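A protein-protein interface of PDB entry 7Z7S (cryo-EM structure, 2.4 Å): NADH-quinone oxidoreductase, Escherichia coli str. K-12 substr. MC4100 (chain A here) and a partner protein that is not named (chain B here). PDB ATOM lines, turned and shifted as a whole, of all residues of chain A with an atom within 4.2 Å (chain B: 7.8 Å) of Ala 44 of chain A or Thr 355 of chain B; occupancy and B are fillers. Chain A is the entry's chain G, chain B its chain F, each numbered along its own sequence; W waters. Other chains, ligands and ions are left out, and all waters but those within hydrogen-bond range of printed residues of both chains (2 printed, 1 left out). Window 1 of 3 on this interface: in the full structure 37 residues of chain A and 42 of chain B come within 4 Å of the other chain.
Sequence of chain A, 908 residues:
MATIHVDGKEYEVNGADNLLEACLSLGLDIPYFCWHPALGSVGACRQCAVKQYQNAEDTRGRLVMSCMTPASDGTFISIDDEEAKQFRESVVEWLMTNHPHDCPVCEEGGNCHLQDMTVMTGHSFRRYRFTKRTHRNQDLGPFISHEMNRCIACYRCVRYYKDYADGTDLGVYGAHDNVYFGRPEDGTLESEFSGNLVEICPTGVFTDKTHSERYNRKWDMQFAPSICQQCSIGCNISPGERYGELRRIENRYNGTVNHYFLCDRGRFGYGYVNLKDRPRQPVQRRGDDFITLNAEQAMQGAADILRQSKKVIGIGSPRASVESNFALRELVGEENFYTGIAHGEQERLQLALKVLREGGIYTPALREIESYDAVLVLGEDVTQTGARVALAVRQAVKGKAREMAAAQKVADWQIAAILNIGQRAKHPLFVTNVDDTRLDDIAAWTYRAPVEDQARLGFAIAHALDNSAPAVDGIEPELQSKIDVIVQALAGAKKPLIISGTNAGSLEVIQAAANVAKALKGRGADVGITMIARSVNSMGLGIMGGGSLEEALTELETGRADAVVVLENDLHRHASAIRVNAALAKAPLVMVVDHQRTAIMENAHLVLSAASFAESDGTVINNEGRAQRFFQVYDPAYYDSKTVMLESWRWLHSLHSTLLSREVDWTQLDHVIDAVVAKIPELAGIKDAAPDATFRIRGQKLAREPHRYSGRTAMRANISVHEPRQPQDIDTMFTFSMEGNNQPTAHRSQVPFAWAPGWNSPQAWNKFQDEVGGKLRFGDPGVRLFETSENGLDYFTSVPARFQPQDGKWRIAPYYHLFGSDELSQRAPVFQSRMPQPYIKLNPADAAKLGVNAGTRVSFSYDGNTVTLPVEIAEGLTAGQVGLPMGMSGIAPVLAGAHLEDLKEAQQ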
ATOM      1  N   CYS A  34     -23.150 -38.196 -15.635  1.00  0.00           N
ATOM      2  CA  CYS A  34     -24.553 -38.533 -15.439  1.00  0.00           C
ATOM      3  C   CYS A  34     -25.253 -38.968 -16.719  1.00  0.00           C
ATOM      4  O   CYS A  34     -26.255 -39.678 -16.642  1.00  0.00           O
ATOM      5  CB  CYS A  34     -25.292 -37.355 -14.797  1.00  0.00           C
ATOM      6  SG  CYS A  34     -25.565 -35.934 -15.841  1.00  0.00           S
ATOM      7  N   VAL A  42     -29.751 -35.684 -18.324  1.00  0.00           N
ATOM      8  CA  VAL A  42     -30.433 -34.989 -17.237  1.00  0.00           C
ATOM      9  C   VAL A  42     -29.690 -33.760 -16.748  1.00  0.00           C
ATOM     10  O   VAL A  42     -30.290 -32.926 -16.054  1.00  0.00           O
ATOM     11  CB  VAL A  42     -30.708 -35.948 -16.058  1.00  0.00           C
ATOM     12  CG1 VAL A  42     -31.869 -36.854 -16.389  1.00  0.00           C
ATOM     13  CG2 VAL A  42     -29.465 -36.738 -15.696  1.00  0.00           C
ATOM     14  N   GLY A  43     -28.418 -33.579 -17.081  1.00  0.00           N
ATOM     15  CA  GLY A  43     -27.669 -32.409 -16.657  1.00  0.00           C
ATOM     16  C   GLY A  43     -27.359 -32.325 -15.178  1.00  0.00           C
ATOM     17  O   GLY A  43     -27.329 -31.225 -14.622  1.00  0.00           O
ATOM     18  N   ALA A  44     -27.099 -33.457 -14.531  1.00  0.00           N
ATOM     19  CA  ALA A  44     -26.842 -33.464 -13.095  1.00  0.00           C
ATOM     20  C   ALA A  44     -25.386 -33.154 -12.766  1.00  0.00           C
ATOM     21  O   ALA A  44     -25.103 -32.201 -12.045  1.00  0.00           O
ATOM     22  CB  ALA A  44     -27.248 -34.811 -12.489  1.00  0.00           C
ATOM     23  N   CYS A  45     -24.449 -33.936 -13.295  1.00  0.00           N
ATOM     24  CA  CYS A  45     -23.083 -33.890 -12.784  1.00  0.00           C
ATOM     25  C   CYS A  45     -22.337 -32.619 -13.169  1.00  0.00           C
ATOM     26  O   CYS A  45     -21.347 -32.286 -12.517  1.00  0.00           O
ATOM     27  CB  CYS A  45     -22.303 -35.106 -13.271  1.00  0.00           C
ATOM     28  SG  CYS A  45     -21.964 -35.095 -15.016  1.00  0.00           S
ATOM     29  N   ARG A  46     -22.783 -31.921 -14.211  1.00  0.00           N
ATOM     30  CA  ARG A  46     -22.183 -30.695 -14.742  1.00  0.00           C
ATOM     31  C   ARG A  46     -20.754 -30.901 -15.239  1.00  0.00           C
ATOM     32  O   ARG A  46     -20.007 -29.937 -15.394  1.00  0.00           O
ATOM     33  CB  ARG A  46     -22.242 -29.536 -13.736  1.00  0.00           C
ATOM     34  CG  ARG A  46     -23.583 -29.377 -13.037  1.00  0.00           C
ATOM     35  CD  ARG A  46     -24.730 -29.260 -13.990  1.00  0.00           C
ATOM     36  NE  ARG A  46     -24.842 -27.944 -14.594  1.00  0.00           N
ATOM     37  CZ  ARG A  46     -25.838 -27.587 -15.385  1.00  0.00           C
ATOM     38  NH1 ARG A  46     -26.818 -28.423 -15.672  1.00  0.00           N
ATOM     39  NH2 ARG A  46     -25.846 -26.367 -15.909  1.00  0.00           N
ATOM     40  N   VAL A  91     -15.069 -29.412 -11.511  1.00  0.00           N
ATOM     41  CA  VAL A  91     -16.105 -30.396 -11.211  1.00  0.00           C
ATOM     42  C   VAL A  91     -15.481 -31.689 -10.703  1.00  0.00           C
ATOM     43  O   VAL A  91     -15.947 -32.270  -9.710  1.00  0.00           O
ATOM     44  CB  VAL A  91     -17.001 -30.637 -12.441  1.00  0.00           C
ATOM     45  CG1 VAL A  91     -17.941 -31.803 -12.200  1.00  0.00           C
ATOM     46  CG2 VAL A  91     -17.797 -29.399 -12.758  1.00  0.00           C
ATOM     47  N   TRP A  94     -14.292 -31.020  -7.147  1.00  0.00           N
ATOM     48  CA  TRP A  94     -15.411 -31.040  -6.209  1.00  0.00           C
ATOM     49  C   TRP A  94     -15.846 -32.462  -5.898  1.00  0.00           C
ATOM     50  O   TRP A  94     -16.183 -32.776  -4.754  1.00  0.00           O
ATOM     51  CB  TRP A  94     -16.586 -30.247  -6.765  1.00  0.00           C
ATOM     52  CG  TRP A  94     -16.376 -28.786  -6.776  1.00  0.00           C
ATOM     53  CD1 TRP A  94     -15.720 -28.045  -5.842  1.00  0.00           C
ATOM     54  CD2 TRP A  94     -16.815 -27.872  -7.778  1.00  0.00           C
ATOM     55  NE1 TRP A  94     -15.725 -26.727  -6.200  1.00  0.00           N
ATOM     56  CE2 TRP A  94     -16.392 -26.592  -7.387  1.00  0.00           C
ATOM     57  CE3 TRP A  94     -17.525 -28.012  -8.969  1.00  0.00           C
ATOM     58  CZ2 TRP A  94     -16.655 -25.461  -8.145  1.00  0.00           C
ATOM     59  CZ3 TRP A  94     -17.782 -26.891  -9.720  1.00  0.00           C
ATOM     60  CH2 TRP A  94     -17.354 -25.630  -9.305  1.00  0.00           C
ATOM     61  N   LEU A  95     -15.856 -33.334  -6.908  1.00  0.00           N
ATOM     62  CA  LEU A  95     -16.164 -34.737  -6.654  1.00  0.00           C
ATOM     63  C   LEU A  95     -15.089 -35.409  -5.807  1.00  0.00           C
ATOM     64  O   LEU A  95     -15.401 -36.294  -5.009  1.00  0.00           O
ATOM     65  CB  LEU A  95     -16.354 -35.482  -7.972  1.00  0.00           C
ATOM     66  CG  LEU A  95     -17.599 -35.067  -8.755  1.00  0.00           C
ATOM     67  CD1 LEU A  95     -17.662 -35.788 -10.078  1.00  0.00           C
ATOM     68  CD2 LEU A  95     -18.848 -35.322  -7.939  1.00  0.00           C
ATOM     69  N   SER B 199     -35.025 -28.966 -15.786  1.00  0.00           N
ATOM     70  CA  SER B 199     -34.436 -28.170 -16.849  1.00  0.00           C
ATOM     71  C   SER B 199     -35.522 -27.443 -17.626  1.00  0.00           C
ATOM     72  O   SER B 199     -36.625 -27.959 -17.817  1.00  0.00           O
ATOM     73  CB  SER B 199     -33.629 -29.052 -17.794  1.00  0.00           C
ATOM     74  OG  SER B 199     -33.635 -30.394 -17.363  1.00  0.00           O
ATOM     75  N   SER B 350     -29.119 -26.995  -0.273  1.00  0.00           N
ATOM     76  CA  SER B 350     -28.906 -27.589  -1.581  1.00  0.00           C
ATOM     77  C   SER B 350     -29.796 -28.814  -1.740  1.00  0.00           C
ATOM     78  O   SER B 350     -29.987 -29.584  -0.801  1.00  0.00           O
ATOM     79  CB  SER B 350     -27.439 -27.977  -1.731  1.00  0.00           C
ATOM     80  OG  SER B 350     -27.211 -28.711  -2.914  1.00  0.00           O
ATOM     81  N   GLY B 352     -29.046 -31.205  -3.787  1.00  0.00           N
ATOM     82  CA  GLY B 352     -28.147 -32.303  -4.046  1.00  0.00           C
ATOM     83  C   GLY B 352     -28.139 -32.823  -5.460  1.00  0.00           C
ATOM     84  O   GLY B 352     -27.501 -33.847  -5.715  1.00  0.00           O
ATOM     85  N   TRP B 353     -28.831 -32.162  -6.385  1.00  0.00           N
ATOM     86  CA  TRP B 353     -28.894 -32.652  -7.755  1.00  0.00           C
ATOM     87  C   TRP B 353     -27.564 -32.475  -8.475  1.00  0.00           C
ATOM     88  O   TRP B 353     -27.072 -33.407  -9.118  1.00  0.00           O
ATOM     89  CB  TRP B 353     -30.013 -31.941  -8.510  1.00  0.00           C
ATOM     90  CG  TRP B 353     -30.149 -32.299  -9.945  1.00  0.00           C
ATOM     91  CD1 TRP B 353     -29.962 -31.476 -11.003  1.00  0.00           C
ATOM     92  CD2 TRP B 353     -30.528 -33.566 -10.483  1.00  0.00           C
ATOM     93  NE1 TRP B 353     -30.193 -32.146 -12.172  1.00  0.00           N
ATOM     94  CE2 TRP B 353     -30.544 -33.435 -11.879  1.00  0.00           C
ATOM     95  CE3 TRP B 353     -30.851 -34.802  -9.919  1.00  0.00           C
ATOM     96  CZ2 TRP B 353     -30.866 -34.490 -12.723  1.00  0.00           C
ATOM     97  CZ3 TRP B 353     -31.170 -35.844 -10.754  1.00  0.00           C
ATOM     98  CH2 TRP B 353     -31.176 -35.684 -12.141  1.00  0.00           C
ATOM     99  N   CYS B 354     -26.955 -31.301  -8.376  1.00  0.00           N
ATOM    100  CA  CYS B 354     -25.840 -30.975  -9.244  1.00  0.00           C
ATOM    101  C   CYS B 354     -24.571 -30.673  -8.458  1.00  0.00           C
ATOM    102  O   CYS B 354     -24.615 -30.065  -7.387  1.00  0.00           O
ATOM    103  CB  CYS B 354     -26.206 -29.826 -10.198  1.00  0.00           C
ATOM    104  SG  CYS B 354     -26.169 -28.166  -9.587  1.00  0.00           S
ATOM    105  N   THR B 355     -23.447 -31.121  -9.027  1.00  0.00           N
ATOM    106  CA  THR B 355     -22.151 -31.114  -8.348  1.00  0.00           C
ATOM    107  C   THR B 355     -21.680 -29.754  -7.834  1.00  0.00           C
ATOM    108  O   THR B 355     -21.253 -29.699  -6.671  1.00  0.00           O
ATOM    109  CB  THR B 355     -21.092 -31.731  -9.271  1.00  0.00           C
ATOM    110  OG1 THR B 355     -21.479 -33.059  -9.628  1.00  0.00           O
ATOM    111  CG2 THR B 355     -19.738 -31.783  -8.584  1.00  0.00           C
ATOM    112  N   PRO B 356     -21.697 -28.648  -8.609  1.00  0.00           N
ATOM    113  CA  PRO B 356     -21.086 -27.407  -8.090  1.00  0.00           C
ATOM    114  C   PRO B 356     -21.736 -26.891  -6.825  1.00  0.00           C
ATOM    115  O   PRO B 356     -21.032 -26.604  -5.865  1.00  0.00           O
ATOM    116  CB  PRO B 356     -21.252 -26.424  -9.255  1.00  0.00           C
ATOM    117  CG  PRO B 356     -21.425 -27.256 -10.425  1.00  0.00           C
ATOM    118  CD  PRO B 356     -22.248 -28.384  -9.944  1.00  0.00           C
ATOM    119  N   CYS B 357     -23.061 -26.857  -6.764  1.00  0.00           N
ATOM    120  CA  CYS B 357     -23.726 -26.405  -5.551  1.00  0.00           C
ATOM    121  C   CYS B 357     -23.508 -27.386  -4.405  1.00  0.00           C
ATOM    122  O   CYS B 357     -22.925 -27.018  -3.378  1.00  0.00           O
ATOM    123  CB  CYS B 357     -25.202 -26.193  -5.851  1.00  0.00           C
ATOM    124  SG  CYS B 357     -26.385 -26.119  -4.520  1.00  0.00           S
ATOM    125  N   ARG B 358     -23.827 -28.665  -4.641  1.00  0.00           N
ATOM    126  CA  ARG B 358     -23.842 -29.685  -3.593  1.00  0.00           C
ATOM    127  C   ARG B 358     -22.461 -29.907  -2.986  1.00  0.00           C
ATOM    128  O   ARG B 358     -22.339 -30.143  -1.781  1.00  0.00           O
ATOM    129  CB  ARG B 358     -24.398 -30.998  -4.157  1.00  0.00           C
ATOM    130  CG  ARG B 358     -23.918 -32.261  -3.459  1.00  0.00           C
ATOM    131  CD  ARG B 358     -24.379 -33.534  -4.125  1.00  0.00           C
ATOM    132  NE  ARG B 358     -23.335 -34.033  -5.007  1.00  0.00           N
ATOM    133  CZ  ARG B 358     -23.425 -34.056  -6.327  1.00  0.00           C
ATOM    134  NH1 ARG B 358     -24.531 -33.690  -6.949  1.00  0.00           N
ATOM    135  NH2 ARG B 358     -22.378 -34.451  -7.040  1.00  0.00           N
ATOM    136  N   ASP B 359     -21.407 -29.821  -3.793  1.00  0.00           N
ATOM    137  CA  ASP B 359     -20.063 -30.112  -3.322  1.00  0.00           C
ATOM    138  C   ASP B 359     -19.155 -28.895  -3.248  1.00  0.00           C
ATOM    139  O   ASP B 359     -18.042 -29.017  -2.738  1.00  0.00           O
ATOM    140  CB  ASP B 359     -19.411 -31.174  -4.210  1.00  0.00           C
ATOM    141  CG  ASP B 359     -19.920 -32.568  -3.920  1.00  0.00           C
ATOM    142  OD1 ASP B 359     -20.245 -32.858  -2.754  1.00  0.00           O
ATOM    143  OD2 ASP B 359     -19.990 -33.381  -4.859  1.00  0.00           O
ATOM    144  N   GLY B 360     -19.592 -27.722  -3.694  1.00  0.00           N
ATOM    145  CA  GLY B 360     -18.735 -26.567  -3.652  1.00  0.00           C
ATOM    146  C   GLY B 360     -19.193 -25.578  -2.612  1.00  0.00           C
ATOM    147  O   GLY B 360     -18.359 -24.872  -2.045  1.00  0.00           O
ATOM    148  N   LEU B 361     -20.500 -25.500  -2.352  1.00  0.00           N
ATOM    149  CA  LEU B 361     -20.954 -24.718  -1.207  1.00  0.00           C
ATOM    150  C   LEU B 361     -20.424 -25.225   0.139  1.00  0.00           C
ATOM    151  O   LEU B 361     -20.044 -24.376   0.963  1.00  0.00           O
ATOM    152  CB  LEU B 361     -22.486 -24.628  -1.226  1.00  0.00           C
ATOM    153  CG  LEU B 361     -23.063 -23.764  -2.342  1.00  0.00           C
ATOM    154  CD1 LEU B 361     -24.575 -23.754  -2.296  1.00  0.00           C
ATOM    155  CD2 LEU B 361     -22.513 -22.357  -2.241  1.00  0.00           C
ATOM    156  N   PRO B 362     -20.375 -26.536   0.443  1.00  0.00           N
ATOM    157  CA  PRO B 362     -19.728 -26.952   1.701  1.00  0.00           C
ATOM    158  C   PRO B 362     -18.249 -26.622   1.789  1.00  0.00           C
ATOM    159  O   PRO B 362     -17.753 -26.380   2.896  1.00  0.00           O
ATOM    160  CB  PRO B 362     -19.959 -28.467   1.724  1.00  0.00           C
ATOM    161  CG  PRO B 362     -21.142 -28.667   0.934  1.00  0.00           C
ATOM    162  CD  PRO B 362     -21.043 -27.694  -0.179  1.00  0.00           C
ATOM    163  N   LEU B 387     -14.736 -20.279  -6.546  1.00  0.00           N
ATOM    164  CA  LEU B 387     -16.041 -20.877  -6.288  1.00  0.00           C
ATOM    165  C   LEU B 387     -17.166 -19.937  -6.691  1.00  0.00           C
ATOM    166  O   LEU B 387     -18.192 -20.379  -7.213  1.00  0.00           O
ATOM    167  CB  LEU B 387     -16.168 -21.253  -4.814  1.00  0.00           C
ATOM    168  CG  LEU B 387     -15.736 -22.665  -4.432  1.00  0.00           C
ATOM    169  CD1 LEU B 387     -15.608 -22.805  -2.927  1.00  0.00           C
ATOM    170  CD2 LEU B 387     -16.718 -23.678  -4.986  1.00  0.00           C
ATOM    171  N   LEU B 391     -19.719 -21.063  -9.771  1.00  0.00           N
ATOM    172  CA  LEU B 391     -21.078 -21.372  -9.353  1.00  0.00           C
ATOM    173  C   LEU B 391     -22.071 -20.346  -9.875  1.00  0.00           C
ATOM    174  O   LEU B 391     -23.199 -20.274  -9.386  1.00  0.00           O
ATOM    175  CB  LEU B 391     -21.167 -21.468  -7.832  1.00  0.00           C
ATOM    176  CG  LEU B 391     -21.040 -22.847  -7.190  1.00  0.00           C
ATOM    177  CD1 LEU B 391     -19.667 -23.448  -7.421  1.00  0.00           C
ATOM    178  CD2 LEU B 391     -21.317 -22.744  -5.716  1.00  0.00           C
ATOM    179  N   LYS B 395     -23.665 -22.447 -14.764  1.00  0.00           N
ATOM    180  CA  LYS B 395     -22.777 -23.510 -14.309  1.00  0.00           C
ATOM    181  C   LYS B 395     -23.535 -24.574 -13.536  1.00  0.00           C
ATOM    182  O   LYS B 395     -23.185 -25.755 -13.604  1.00  0.00           O
ATOM    183  CB  LYS B 395     -21.660 -22.938 -13.441  1.00  0.00           C
ATOM    184  CG  LYS B 395     -21.016 -21.691 -13.978  1.00  0.00           C
ATOM    185  CD  LYS B 395     -20.066 -22.001 -15.099  1.00  0.00           C
ATOM    186  CE  LYS B 395     -19.150 -20.827 -15.363  1.00  0.00           C
ATOM    187  NZ  LYS B 395     -19.912 -19.566 -15.502  1.00  0.00           N
ATOM    188  N   THR B 396     -24.556 -24.180 -12.793  1.00  0.00           N
ATOM    189  CA  THR B 396     -25.351 -25.102 -12.004  1.00  0.00           C
ATOM    190  C   THR B 396     -26.696 -25.347 -12.669  1.00  0.00           C
ATOM    191  O   THR B 396     -27.078 -24.680 -13.630  1.00  0.00           O
ATOM    192  CB  THR B 396     -25.543 -24.571 -10.584  1.00  0.00           C
ATOM    193  OG1 THR B 396     -26.275 -23.346 -10.627  1.00  0.00           O
ATOM    194  CG2 THR B 396     -24.208 -24.327  -9.939  1.00  0.00           C
ATOM    195  N   PHE B 397     -27.417 -26.326 -12.134  1.00  0.00           N
ATOM    196  CA  PHE B 397     -28.666 -26.754 -12.750  1.00  0.00           C
ATOM    197  C   PHE B 397     -29.781 -25.744 -12.520  1.00  0.00           C
ATOM    198  O   PHE B 397     -30.636 -25.554 -13.391  1.00  0.00           O
ATOM    199  CB  PHE B 397     -29.054 -28.124 -12.214  1.00  0.00           C
ATOM    200  CG  PHE B 397     -30.169 -28.775 -12.961  1.00  0.00           C
ATOM    201  CD1 PHE B 397     -29.935 -29.410 -14.163  1.00  0.00           C
ATOM    202  CD2 PHE B 397     -31.453 -28.767 -12.453  1.00  0.00           C
ATOM    203  CE1 PHE B 397     -30.958 -30.017 -14.842  1.00  0.00           C
ATOM    204  CE2 PHE B 397     -32.474 -29.370 -13.131  1.00  0.00           C
ATOM    205  CZ  PHE B 397     -32.229 -29.996 -14.323  1.00  0.00           C
HETATM  206  O   HOH W   1     -33.138 -32.892 -16.364  1.00  0.00           O
HETATM  207  O   HOH W   2     -24.582 -34.507  -9.683  1.00  0.00           O
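Among the printed residues, merely in contact across the chains: Val 42 of chain A with Trp 353 of chain B (3.6 Å), Val 42 of chain A with Phe 397 of chain B (3.2 Å), Gly 43 of chain A with Trp 353 of chain B (3.9 Å), Gly 43 of chain A with Phe 397 of chain B (3.2 Å), Ala 44 of chain A with Trp 353 of chain B (3.6 Å), Ala 44 of chain A with Cys 354 of chain B (3.1 Å), Ala 44 of chain A with Thr 355 of chain B (3.6 Å), Arg 46 of chain A with Cys 354 of chain B (3.9 Å), Arg 46 of chain A with Pro 356 of chain B (3.5 Å), Arg 46 of chain A with Phe 397 of chain B (3.6 Å), Val 91 of chain A with Thr 355 of chain B (3.98 Å), Trp 94 of chain A with Thr 355 of chain B (3.95 Å), Trp 94 of chain A with Pro 356 of chain B (3.5 Å), Trp 94 of chain A with Asp 359 of chain B (3.6 Å), Trp 94 of chain A with Gly 360 of chain B (3.9 Å), Trp 94 of chain A with Leu 387 of chain B (3.4 Å), Trp 94 of chain A with Leu 391 of chain B (3.7 Å), Leu 95 of chain A with Thr 355 of chain B (3.7 Å), Leu 95 of chain A with Arg 358 of chain B (3.7 Å) and Leu 95 of chain A with Asp 359 of chain B (3.8 Å).
Hydrophobic or aromatic side chains of chain A within 4 Å of the printed part of chain B: Val 42, Ala 44, Trp 94 and Leu 95.
Of the 18 printed residues of chain B, 12 touch a printed residue of chain A.
Hydrophobic or aromatic side chains of chain B that line the printed part of chain A: Trp 353, Pro 356, Leu 387, Leu 391 and Phe 397.
Among the printed residues, 23 pairs touch across the chains.
Among the printed residues, no Asp or Glu carboxylate lies within 4 Å of a Lys or Arg side-chain nitrogen of the other chain.
The side-chain sulfur (SG) of Cys 34 of chain A sits close to the backbone NH (N) of Ala 44 of chain A.
The backbone carbonyl oxygen (O) of Gly 43 of chain A sits at hydrogen-bond distance from the guanidinium group (NH1) of Arg 46 of chain A (3.0 Å).
The guanidinium group (NH1) of Arg 358 of chain B lies within hydrogen-bond range of the backbone carbonyl oxygen (O) of Gly 352 of chain B (3.2 Å).
The side-chain hydroxyl (OG1) of Thr 355 of chain B is in hydrogen-bond range of the guanidinium group (NH2) of Arg 358 of chain B, 3.1 Å away.
The backbone carbonyl oxygen of Trp 353 of chain B is in hydrogen-bond range of the guanidinium group of Arg 358 of chain B (3.4 Å).
NH2 of Arg 358 of chain B lies within salt-bridge range of OD2 of Asp 359 of chain B (3.4 Å).
Of chain B, only Trp 353 and Phe 397 come within 4 Å of Gly 43 of chain A.
Of chain B, only Trp 353, Cys 354 and Thr 355 come within 4 Å of Ala 44 of chain A.
Printed residues of chain B within 4 Å of Val 91 of chain A: Thr 355.
Ser 350 of chain B touches none of the printed residues of chain A.
Gly 352 of chain B touches none of the printed residues of chain A.
Printed residues of chain A within 4 Å of Thr 355 of chain B: Ala 44, Cys 45, Val 91, Trp 94 and Leu 95.
Of the printed residues of chain A, Pro 356 of chain B touches Arg 46 and Trp 94.
Of the printed residues of chain A, Gly 360 of chain B touches Trp 94.
Of the printed residues of chain A, Leu 387 of chain B touches Trp 94 (3.4 Å).
O of Thr 396 of chain B lies within hydrogen-bond range of NH2 of Arg 46 of chain A (3.1 Å).
The backbone carbonyl oxygen (O) of Lys 395 of chain B sits at hydrogen-bond distance from the guanidinium group (NE) of Arg 46 of chain A.
The backbone carbonyl oxygen (O) of Cys 45 of chain A is in hydrogen-bond range of the side-chain hydroxyl (OG1) of Thr 355 of chain B (3.0 Å).
Water W1 bridges OG of Ser 199 of chain B and O of Val 42 of chain A.
Water W2 lies within hydrogen-bond range of O of Trp 353 of chain B (2.8 Å), NH1 of Arg 358 of chain B (2.9 Å), O of Ala 44 of chain A (3.3 Å) and OG1 of Thr 355 of chain B (3.4 Å).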
